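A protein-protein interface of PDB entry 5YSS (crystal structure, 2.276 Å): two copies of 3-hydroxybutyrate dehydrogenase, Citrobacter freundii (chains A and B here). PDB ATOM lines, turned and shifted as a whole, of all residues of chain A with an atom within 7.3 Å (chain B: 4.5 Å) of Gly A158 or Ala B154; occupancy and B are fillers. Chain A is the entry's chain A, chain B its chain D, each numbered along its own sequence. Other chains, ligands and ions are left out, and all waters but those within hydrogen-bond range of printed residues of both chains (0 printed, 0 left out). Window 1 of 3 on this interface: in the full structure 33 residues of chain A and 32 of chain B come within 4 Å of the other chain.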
ATOM      1  N   ASN A 111     -11.636  21.337  23.120  1.00  0.00           N
ATOM      2  CA  ASN A 111     -11.835  22.783  23.062  1.00  0.00           C
ATOM      3  C   ASN A 111     -12.521  23.267  21.782  1.00  0.00           C
ATOM      4  O   ASN A 111     -13.006  24.394  21.744  1.00  0.00           O
ATOM      5  CB  ASN A 111     -10.497  23.525  23.210  1.00  0.00           C
ATOM      6  CG  ASN A 111      -9.789  23.233  24.532  1.00  0.00           C
ATOM      7  OD1 ASN A 111     -10.141  22.305  25.261  1.00  0.00           O
ATOM      8  ND2 ASN A 111      -8.767  24.027  24.831  1.00  0.00           N
ATOM      9  N   LEU A 112     -12.558  22.438  20.739  1.00  0.00           N
ATOM     10  CA  LEU A 112     -13.166  22.860  19.481  1.00  0.00           C
ATOM     11  C   LEU A 112     -14.317  21.968  18.999  1.00  0.00           C
ATOM     12  O   LEU A 112     -15.439  22.433  18.861  1.00  0.00           O
ATOM     13  CB  LEU A 112     -12.112  22.939  18.382  1.00  0.00           C
ATOM     14  CG  LEU A 112     -12.677  23.372  17.025  1.00  0.00           C
ATOM     15  CD1 LEU A 112     -13.415  24.683  17.176  1.00  0.00           C
ATOM     16  CD2 LEU A 112     -11.580  23.498  15.948  1.00  0.00           C
ATOM     17  N   HIS A 141      -7.229  34.145  23.614  1.00  0.00           N
ATOM     18  CA  HIS A 141      -6.403  33.385  22.688  1.00  0.00           C
ATOM     19  C   HIS A 141      -7.185  32.922  21.464  1.00  0.00           C
ATOM     20  O   HIS A 141      -6.664  32.185  20.616  1.00  0.00           O
ATOM     21  CB  HIS A 141      -5.772  32.188  23.394  1.00  0.00           C
ATOM     22  CG  HIS A 141      -4.629  32.563  24.278  1.00  0.00           C
ATOM     23  ND1 HIS A 141      -4.725  32.607  25.654  1.00  0.00           N
ATOM     24  CD2 HIS A 141      -3.371  32.964  23.978  1.00  0.00           C
ATOM     25  CE1 HIS A 141      -3.570  32.989  26.163  1.00  0.00           C
ATOM     26  NE2 HIS A 141      -2.732  33.210  25.165  1.00  0.00           N
ATOM     27  N   GLY A 142      -8.436  33.356  21.388  1.00  0.00           N
ATOM     28  CA  GLY A 142      -9.229  33.144  20.204  1.00  0.00           C
ATOM     29  C   GLY A 142      -9.036  34.349  19.315  1.00  0.00           C
ATOM     30  O   GLY A 142      -9.456  34.338  18.160  1.00  0.00           O
ATOM     31  N   TYR A 152      -4.002  25.148  21.803  1.00  0.00           N
ATOM     32  CA  TYR A 152      -5.025  25.934  22.472  1.00  0.00           C
ATOM     33  C   TYR A 152      -5.452  27.196  21.691  1.00  0.00           C
ATOM     34  O   TYR A 152      -6.640  27.536  21.652  1.00  0.00           O
ATOM     35  CB  TYR A 152      -4.513  26.315  23.849  1.00  0.00           C
ATOM     36  CG  TYR A 152      -5.468  27.036  24.766  1.00  0.00           C
ATOM     37  CD1 TYR A 152      -6.297  26.340  25.635  1.00  0.00           C
ATOM     38  CD2 TYR A 152      -5.486  28.423  24.812  1.00  0.00           C
ATOM     39  CE1 TYR A 152      -7.142  27.020  26.511  1.00  0.00           C
ATOM     40  CE2 TYR A 152      -6.322  29.104  25.673  1.00  0.00           C
ATOM     41  CZ  TYR A 152      -7.142  28.406  26.517  1.00  0.00           C
ATOM     42  OH  TYR A 152      -7.955  29.117  27.365  1.00  0.00           O
ATOM     43  N   VAL A 153      -4.489  27.897  21.100  1.00  0.00           N
ATOM     44  CA  VAL A 153      -4.767  29.091  20.300  1.00  0.00           C
ATOM     45  C   VAL A 153      -5.524  28.722  19.016  1.00  0.00           C
ATOM     46  O   VAL A 153      -6.460  29.415  18.606  1.00  0.00           O
ATOM     47  CB  VAL A 153      -3.455  29.845  19.942  1.00  0.00           C
ATOM     48  CG1 VAL A 153      -3.715  31.026  19.003  1.00  0.00           C
ATOM     49  CG2 VAL A 153      -2.737  30.314  21.212  1.00  0.00           C
ATOM     50  N   ALA A 154      -5.120  27.615  18.402  1.00  0.00           N
ATOM     51  CA  ALA A 154      -5.759  27.135  17.186  1.00  0.00           C
ATOM     52  C   ALA A 154      -7.208  26.739  17.460  1.00  0.00           C
ATOM     53  O   ALA A 154      -8.115  27.072  16.686  1.00  0.00           O
ATOM     54  CB  ALA A 154      -4.991  25.959  16.606  1.00  0.00           C
ATOM     55  N   ALA A 155      -7.409  26.021  18.560  1.00  0.00           N
ATOM     56  CA  ALA A 155      -8.733  25.580  18.970  1.00  0.00           C
ATOM     57  C   ALA A 155      -9.659  26.759  19.264  1.00  0.00           C
ATOM     58  O   ALA A 155     -10.839  26.760  18.855  1.00  0.00           O
ATOM     59  CB  ALA A 155      -8.627  24.691  20.186  1.00  0.00           C
ATOM     60  N   LYS A 156      -9.120  27.758  19.969  1.00  0.00           N
ATOM     61  CA  LYS A 156      -9.934  28.867  20.484  1.00  0.00           C
ATOM     62  C   LYS A 156     -10.301  29.830  19.360  1.00  0.00           C
ATOM     63  O   LYS A 156     -11.445  30.279  19.268  1.00  0.00           O
ATOM     64  CB  LYS A 156      -9.204  29.610  21.610  1.00  0.00           C
ATOM     65  CG  LYS A 156      -9.127  28.836  22.915  1.00  0.00           C
ATOM     66  CD  LYS A 156     -10.532  28.478  23.451  1.00  0.00           C
ATOM     67  CE  LYS A 156     -10.504  28.269  24.958  1.00  0.00           C
ATOM     68  NZ  LYS A 156     -11.822  27.858  25.552  1.00  0.00           N
ATOM     69  N   HIS A 157      -9.316  30.140  18.520  1.00  0.00           N
ATOM     70  CA  HIS A 157      -9.534  30.824  17.253  1.00  0.00           C
ATOM     71  C   HIS A 157     -10.608  30.090  16.465  1.00  0.00           C
ATOM     72  O   HIS A 157     -11.503  30.706  15.898  1.00  0.00           O
ATOM     73  CB  HIS A 157      -8.239  30.893  16.420  1.00  0.00           C
ATOM     74  CG  HIS A 157      -7.407  32.109  16.685  1.00  0.00           C
ATOM     75  ND1 HIS A 157      -6.651  32.259  17.831  1.00  0.00           N
ATOM     76  CD2 HIS A 157      -7.206  33.232  15.954  1.00  0.00           C
ATOM     77  CE1 HIS A 157      -6.032  33.424  17.797  1.00  0.00           C
ATOM     78  NE2 HIS A 157      -6.354  34.039  16.673  1.00  0.00           N
ATOM     79  N   GLY A 158     -10.501  28.765  16.438  1.00  0.00           N
ATOM     80  CA  GLY A 158     -11.464  27.934  15.748  1.00  0.00           C
ATOM     81  C   GLY A 158     -12.853  28.188  16.296  1.00  0.00           C
ATOM     82  O   GLY A 158     -13.775  28.461  15.512  1.00  0.00           O
ATOM     83  N   VAL A 159     -13.000  28.126  17.627  1.00  0.00           N
ATOM     84  CA  VAL A 159     -14.289  28.365  18.270  1.00  0.00           C
ATOM     85  C   VAL A 159     -14.857  29.705  17.840  1.00  0.00           C
ATOM     86  O   VAL A 159     -16.061  29.829  17.576  1.00  0.00           O
ATOM     87  CB  VAL A 159     -14.198  28.359  19.814  1.00  0.00           C
ATOM     88  CG1 VAL A 159     -15.438  28.987  20.415  1.00  0.00           C
ATOM     89  CG2 VAL A 159     -13.995  26.955  20.336  1.00  0.00           C
ATOM     90  N   VAL A 160     -13.995  30.711  17.760  1.00  0.00           N
ATOM     91  CA  VAL A 160     -14.454  32.037  17.348  1.00  0.00           C
ATOM     92  C   VAL A 160     -15.042  32.006  15.929  1.00  0.00           C
ATOM     93  O   VAL A 160     -16.162  32.458  15.716  1.00  0.00           O
ATOM     94  CB  VAL A 160     -13.317  33.064  17.442  1.00  0.00           C
ATOM     95  CG1 VAL A 160     -13.697  34.363  16.726  1.00  0.00           C
ATOM     96  CG2 VAL A 160     -12.991  33.314  18.917  1.00  0.00           C
ATOM     97  N   GLY A 161     -14.302  31.456  14.967  1.00  0.00           N
ATOM     98  CA  GLY A 161     -14.854  31.256  13.640  1.00  0.00           C
ATOM     99  C   GLY A 161     -16.183  30.497  13.629  1.00  0.00           C
ATOM    100  O   GLY A 161     -17.152  30.941  13.015  1.00  0.00           O
ATOM    101  N   LEU A 162     -16.217  29.354  14.312  1.00  0.00           N
ATOM    102  CA  LEU A 162     -17.406  28.511  14.398  1.00  0.00           C
ATOM    103  C   LEU A 162     -18.613  29.283  14.945  1.00  0.00           C
ATOM    104  O   LEU A 162     -19.739  29.121  14.481  1.00  0.00           O
ATOM    105  CB  LEU A 162     -17.126  27.285  15.276  1.00  0.00           C
ATOM    106  CG  LEU A 162     -18.341  26.384  15.536  1.00  0.00           C
ATOM    107  CD1 LEU A 162     -18.950  25.875  14.223  1.00  0.00           C
ATOM    108  CD2 LEU A 162     -17.949  25.224  16.436  1.00  0.00           C
ATOM    109  N   THR A 163     -18.354  30.129  15.929  1.00  0.00           N
ATOM    110  CA  THR A 163     -19.389  30.933  16.552  1.00  0.00           C
ATOM    111  C   THR A 163     -20.031  31.877  15.542  1.00  0.00           C
ATOM    112  O   THR A 163     -21.252  32.029  15.508  1.00  0.00           O
ATOM    113  CB  THR A 163     -18.818  31.746  17.733  1.00  0.00           C
ATOM    114  OG1 THR A 163     -18.383  30.844  18.753  1.00  0.00           O
ATOM    115  CG2 THR A 163     -19.858  32.670  18.313  1.00  0.00           C
ATOM    116  N   LYS A 164     -19.192  32.521  14.742  1.00  0.00           N
ATOM    117  CA  LYS A 164     -19.649  33.484  13.752  1.00  0.00           C
ATOM    118  C   LYS A 164     -20.528  32.817  12.705  1.00  0.00           C
ATOM    119  O   LYS A 164     -21.540  33.375  12.287  1.00  0.00           O
ATOM    120  CB  LYS A 164     -18.465  34.158  13.062  1.00  0.00           C
ATOM    121  CG  LYS A 164     -17.604  35.048  13.940  1.00  0.00           C
ATOM    122  CD  LYS A 164     -16.401  35.534  13.144  1.00  0.00           C
ATOM    123  CE  LYS A 164     -15.402  36.309  14.002  1.00  0.00           C
ATOM    124  NZ  LYS A 164     -14.116  36.560  13.263  1.00  0.00           N
ATOM    125  N   THR A 165     -20.159  31.616  12.288  1.00  0.00           N
ATOM    126  CA  THR A 165     -20.856  31.008  11.173  1.00  0.00           C
ATOM    127  C   THR A 165     -22.214  30.485  11.670  1.00  0.00           C
ATOM    128  O   THR A 165     -23.210  30.525  10.945  1.00  0.00           O
ATOM    129  CB  THR A 165     -19.993  29.906  10.472  1.00  0.00           C
ATOM    130  OG1 THR A 165     -20.798  29.173   9.536  1.00  0.00           O
ATOM    131  CG2 THR A 165     -19.434  28.950  11.446  1.00  0.00           C
ATOM    132  N   TRP B 104     -16.716  16.847   9.089  1.00  0.00           N
ATOM    133  CA  TRP B 104     -16.131  17.724  10.088  1.00  0.00           C
ATOM    134  C   TRP B 104     -14.720  17.248  10.428  1.00  0.00           C
ATOM    135  O   TRP B 104     -13.783  18.051  10.460  1.00  0.00           O
ATOM    136  CB  TRP B 104     -16.989  17.787  11.348  1.00  0.00           C
ATOM    137  CG  TRP B 104     -16.257  18.403  12.517  1.00  0.00           C
ATOM    138  CD1 TRP B 104     -15.448  17.758  13.403  1.00  0.00           C
ATOM    139  CD2 TRP B 104     -16.258  19.785  12.909  1.00  0.00           C
ATOM    140  NE1 TRP B 104     -14.961  18.641  14.324  1.00  0.00           N
ATOM    141  CE2 TRP B 104     -15.435  19.894  14.042  1.00  0.00           C
ATOM    142  CE3 TRP B 104     -16.887  20.936  12.419  1.00  0.00           C
ATOM    143  CZ2 TRP B 104     -15.213  21.108  14.691  1.00  0.00           C
ATOM    144  CZ3 TRP B 104     -16.666  22.147  13.069  1.00  0.00           C
ATOM    145  CH2 TRP B 104     -15.831  22.220  14.187  1.00  0.00           C
ATOM    146  N   SER B 150     -19.268  25.736   8.544  1.00  0.00           N
ATOM    147  CA  SER B 150     -18.791  25.705   9.927  1.00  0.00           C
ATOM    148  C   SER B 150     -17.427  25.009  10.113  1.00  0.00           C
ATOM    149  O   SER B 150     -16.566  25.519  10.836  1.00  0.00           O
ATOM    150  CB  SER B 150     -19.839  25.049  10.830  1.00  0.00           C
ATOM    151  OG  SER B 150     -20.055  23.698  10.473  1.00  0.00           O
ATOM    152  N   ALA B 151     -17.217  23.868   9.466  1.00  0.00           N
ATOM    153  CA  ALA B 151     -15.970  23.157   9.671  1.00  0.00           C
ATOM    154  C   ALA B 151     -14.822  23.910   8.997  1.00  0.00           C
ATOM    155  O   ALA B 151     -13.705  23.938   9.501  1.00  0.00           O
ATOM    156  CB  ALA B 151     -16.060  21.743   9.146  1.00  0.00           C
ATOM    157  N   TYR B 152     -15.108  24.541   7.869  1.00  0.00           N
ATOM    158  CA  TYR B 152     -14.086  25.243   7.099  1.00  0.00           C
ATOM    159  C   TYR B 152     -13.691  26.565   7.751  1.00  0.00           C
ATOM    160  O   TYR B 152     -12.516  26.898   7.836  1.00  0.00           O
ATOM    161  CB  TYR B 152     -14.603  25.484   5.685  1.00  0.00           C
ATOM    162  CG  TYR B 152     -13.660  26.143   4.710  1.00  0.00           C
ATOM    163  CD1 TYR B 152     -12.860  25.384   3.874  1.00  0.00           C
ATOM    164  CD2 TYR B 152     -13.632  27.524   4.568  1.00  0.00           C
ATOM    165  CE1 TYR B 152     -12.028  25.985   2.946  1.00  0.00           C
ATOM    166  CE2 TYR B 152     -12.808  28.132   3.645  1.00  0.00           C
ATOM    167  CZ  TYR B 152     -12.010  27.359   2.840  1.00  0.00           C
ATOM    168  OH  TYR B 152     -11.192  27.960   1.920  1.00  0.00           O
ATOM    169  N   VAL B 153     -14.682  27.327   8.179  1.00  0.00           N
ATOM    170  CA  VAL B 153     -14.423  28.590   8.854  1.00  0.00           C
ATOM    171  C   VAL B 153     -13.665  28.349  10.156  1.00  0.00           C
ATOM    172  O   VAL B 153     -12.755  29.109  10.502  1.00  0.00           O
ATOM    173  CB  VAL B 153     -15.736  29.346   9.128  1.00  0.00           C
ATOM    174  CG1 VAL B 153     -15.491  30.608   9.961  1.00  0.00           C
ATOM    175  CG2 VAL B 153     -16.442  29.671   7.777  1.00  0.00           C
ATOM    176  N   ALA B 154     -14.017  27.268  10.849  1.00  0.00           N
ATOM    177  CA  ALA B 154     -13.339  26.903  12.093  1.00  0.00           C
ATOM    178  C   ALA B 154     -11.875  26.579  11.839  1.00  0.00           C
ATOM    179  O   ALA B 154     -10.980  27.107  12.508  1.00  0.00           O
ATOM    180  CB  ALA B 154     -14.026  25.716  12.762  1.00  0.00           C
ATOM    181  N   ALA B 155     -11.634  25.698  10.879  1.00  0.00           N
ATOM    182  CA  ALA B 155     -10.298  25.220  10.605  1.00  0.00           C
ATOM    183  C   ALA B 155      -9.411  26.368  10.167  1.00  0.00           C
ATOM    184  O   ALA B 155      -8.253  26.485  10.606  1.00  0.00           O
ATOM    185  CB  ALA B 155     -10.334  24.143   9.557  1.00  0.00           C
ATOM    186  N   LYS B 156      -9.971  27.239   9.335  1.00  0.00           N
ATOM    187  CA  LYS B 156      -9.209  28.348   8.762  1.00  0.00           C
ATOM    188  C   LYS B 156      -8.923  29.394   9.836  1.00  0.00           C
ATOM    189  O   LYS B 156      -7.804  29.901   9.925  1.00  0.00           O
ATOM    190  CB  LYS B 156      -9.958  28.963   7.570  1.00  0.00           C
ATOM    191  CG  LYS B 156     -10.019  28.065   6.315  1.00  0.00           C
ATOM    192  CD  LYS B 156      -8.620  27.869   5.700  1.00  0.00           C
ATOM    193  CE  LYS B 156      -8.674  27.081   4.386  1.00  0.00           C
ATOM    194  NZ  LYS B 156      -7.326  26.681   3.880  1.00  0.00           N
ATOM    195  N   HIS B 157      -9.926  29.716  10.657  1.00  0.00           N
ATOM    196  CA  HIS B 157      -9.655  30.504  11.865  1.00  0.00           C
ATOM    197  C   HIS B 157      -8.562  29.827  12.689  1.00  0.00           C
ATOM    198  O   HIS B 157      -7.630  30.483  13.176  1.00  0.00           O
ATOM    199  CB  HIS B 157     -10.923  30.696  12.715  1.00  0.00           C
ATOM    200  CG  HIS B 157     -11.775  31.841  12.258  1.00  0.00           C
ATOM    201  ND1 HIS B 157     -12.491  31.810  11.080  1.00  0.00           N
ATOM    202  CD2 HIS B 157     -11.978  33.066  12.794  1.00  0.00           C
ATOM    203  CE1 HIS B 157     -13.113  32.967  10.917  1.00  0.00           C
ATOM    204  NE2 HIS B 157     -12.821  33.743  11.943  1.00  0.00           N
ATOM    205  N   GLY B 158      -8.673  28.509  12.820  1.00  0.00           N
ATOM    206  CA  GLY B 158      -7.687  27.728  13.540  1.00  0.00           C
ATOM    207  C   GLY B 158      -6.299  27.909  12.961  1.00  0.00           C
ATOM    208  O   GLY B 158      -5.324  28.037  13.712  1.00  0.00           O
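The side-chain amino group of Lys A164 lies within hydrogen-bond range of a ring nitrogen (NE2) of His B157 (3.4 Å).
A ring nitrogen (ND1) of His A157 is in hydrogen-bond range of the backbone carbonyl oxygen (O) of His A141 (2.8 Å).
NE2 of His A157 sits close to O of Gly A142 (3.5 Å).
A ring nitrogen (ND1) of His A157 sits at hydrogen-bond distance from the backbone carbonyl oxygen of Val A153 (3.0 Å).
The backbone carbonyl oxygen (O) of Val B153 sits at hydrogen-bond distance from a ring nitrogen (ND1) of His B157.
CA of Gly B158 touches O of Ala A154 (3.2 Å).
His B157 touches His A157 (CB to O, 3.2 Å).
O of Ala B154 touches CA of Gly A158 (3.4 Å).
Gly A161 touches Val B153.
His B157 touches Gly A161.
Ser B150 touches Leu A162.
Thr A165 touches Ser B150.
Asn A111 touches none of the printed residues of chain B.
Val A153 touches none of the printed residues of chain B.
Of the printed residues of chain B, His A157 touches His B157.
Gly A158 touches just one residue of chain B: Ala B154.
Of the printed residues of chain B, Gly A161 touches Val B153 (3.5 Å) and His B157 (3.4 Å).
Of the printed residues of chain B, Leu A162 touches Ser B150.
Of the printed residues of chain A, Ser B150 touches Leu A162 (3.6 Å) and Thr A165 (3.6 Å).
Of the printed residues of chain A, Val B153 touches Gly A161 (3.5 Å).
Of chain A, only Gly A158 (3.4 Å) comes within 4 Å of Ala B154.
The nearest residue of chain B that does not touch Gly A158 is Gly B158 (4.1 Å).
Of the 10 printed residues of chain B, 5 touch a printed residue of chain A.
Printed residues of chain B that touch a printed residue of chain A: Ser B150, Val B153, Ala B154, His B157 and Gly B158.
Hydrophobic or aromatic side chains of chain B that line the printed part of chain A: Val B153, Ala B154 and His B157.
Hydrophobic or aromatic side chains of chain A that line the printed part of chain B: Ala A154, His A157 and Leu A162.
Along chain A the printed residues that touch a printed residue of chain B span positions 154 to 165.
Among the printed residues, no Asp or Glu carboxylate lies within 4 Å of a Lys or Arg side-chain nitrogen of the other chain.
Ala A154 touches Gly B158, and with the chains exchanged Gly A158 touches Ala B154.
His B157 touches its own counterpart, His A157.
Of the 8 pairs that touch across the chains among the printed residues, 3 have their exchanged pair printed and touching as well.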
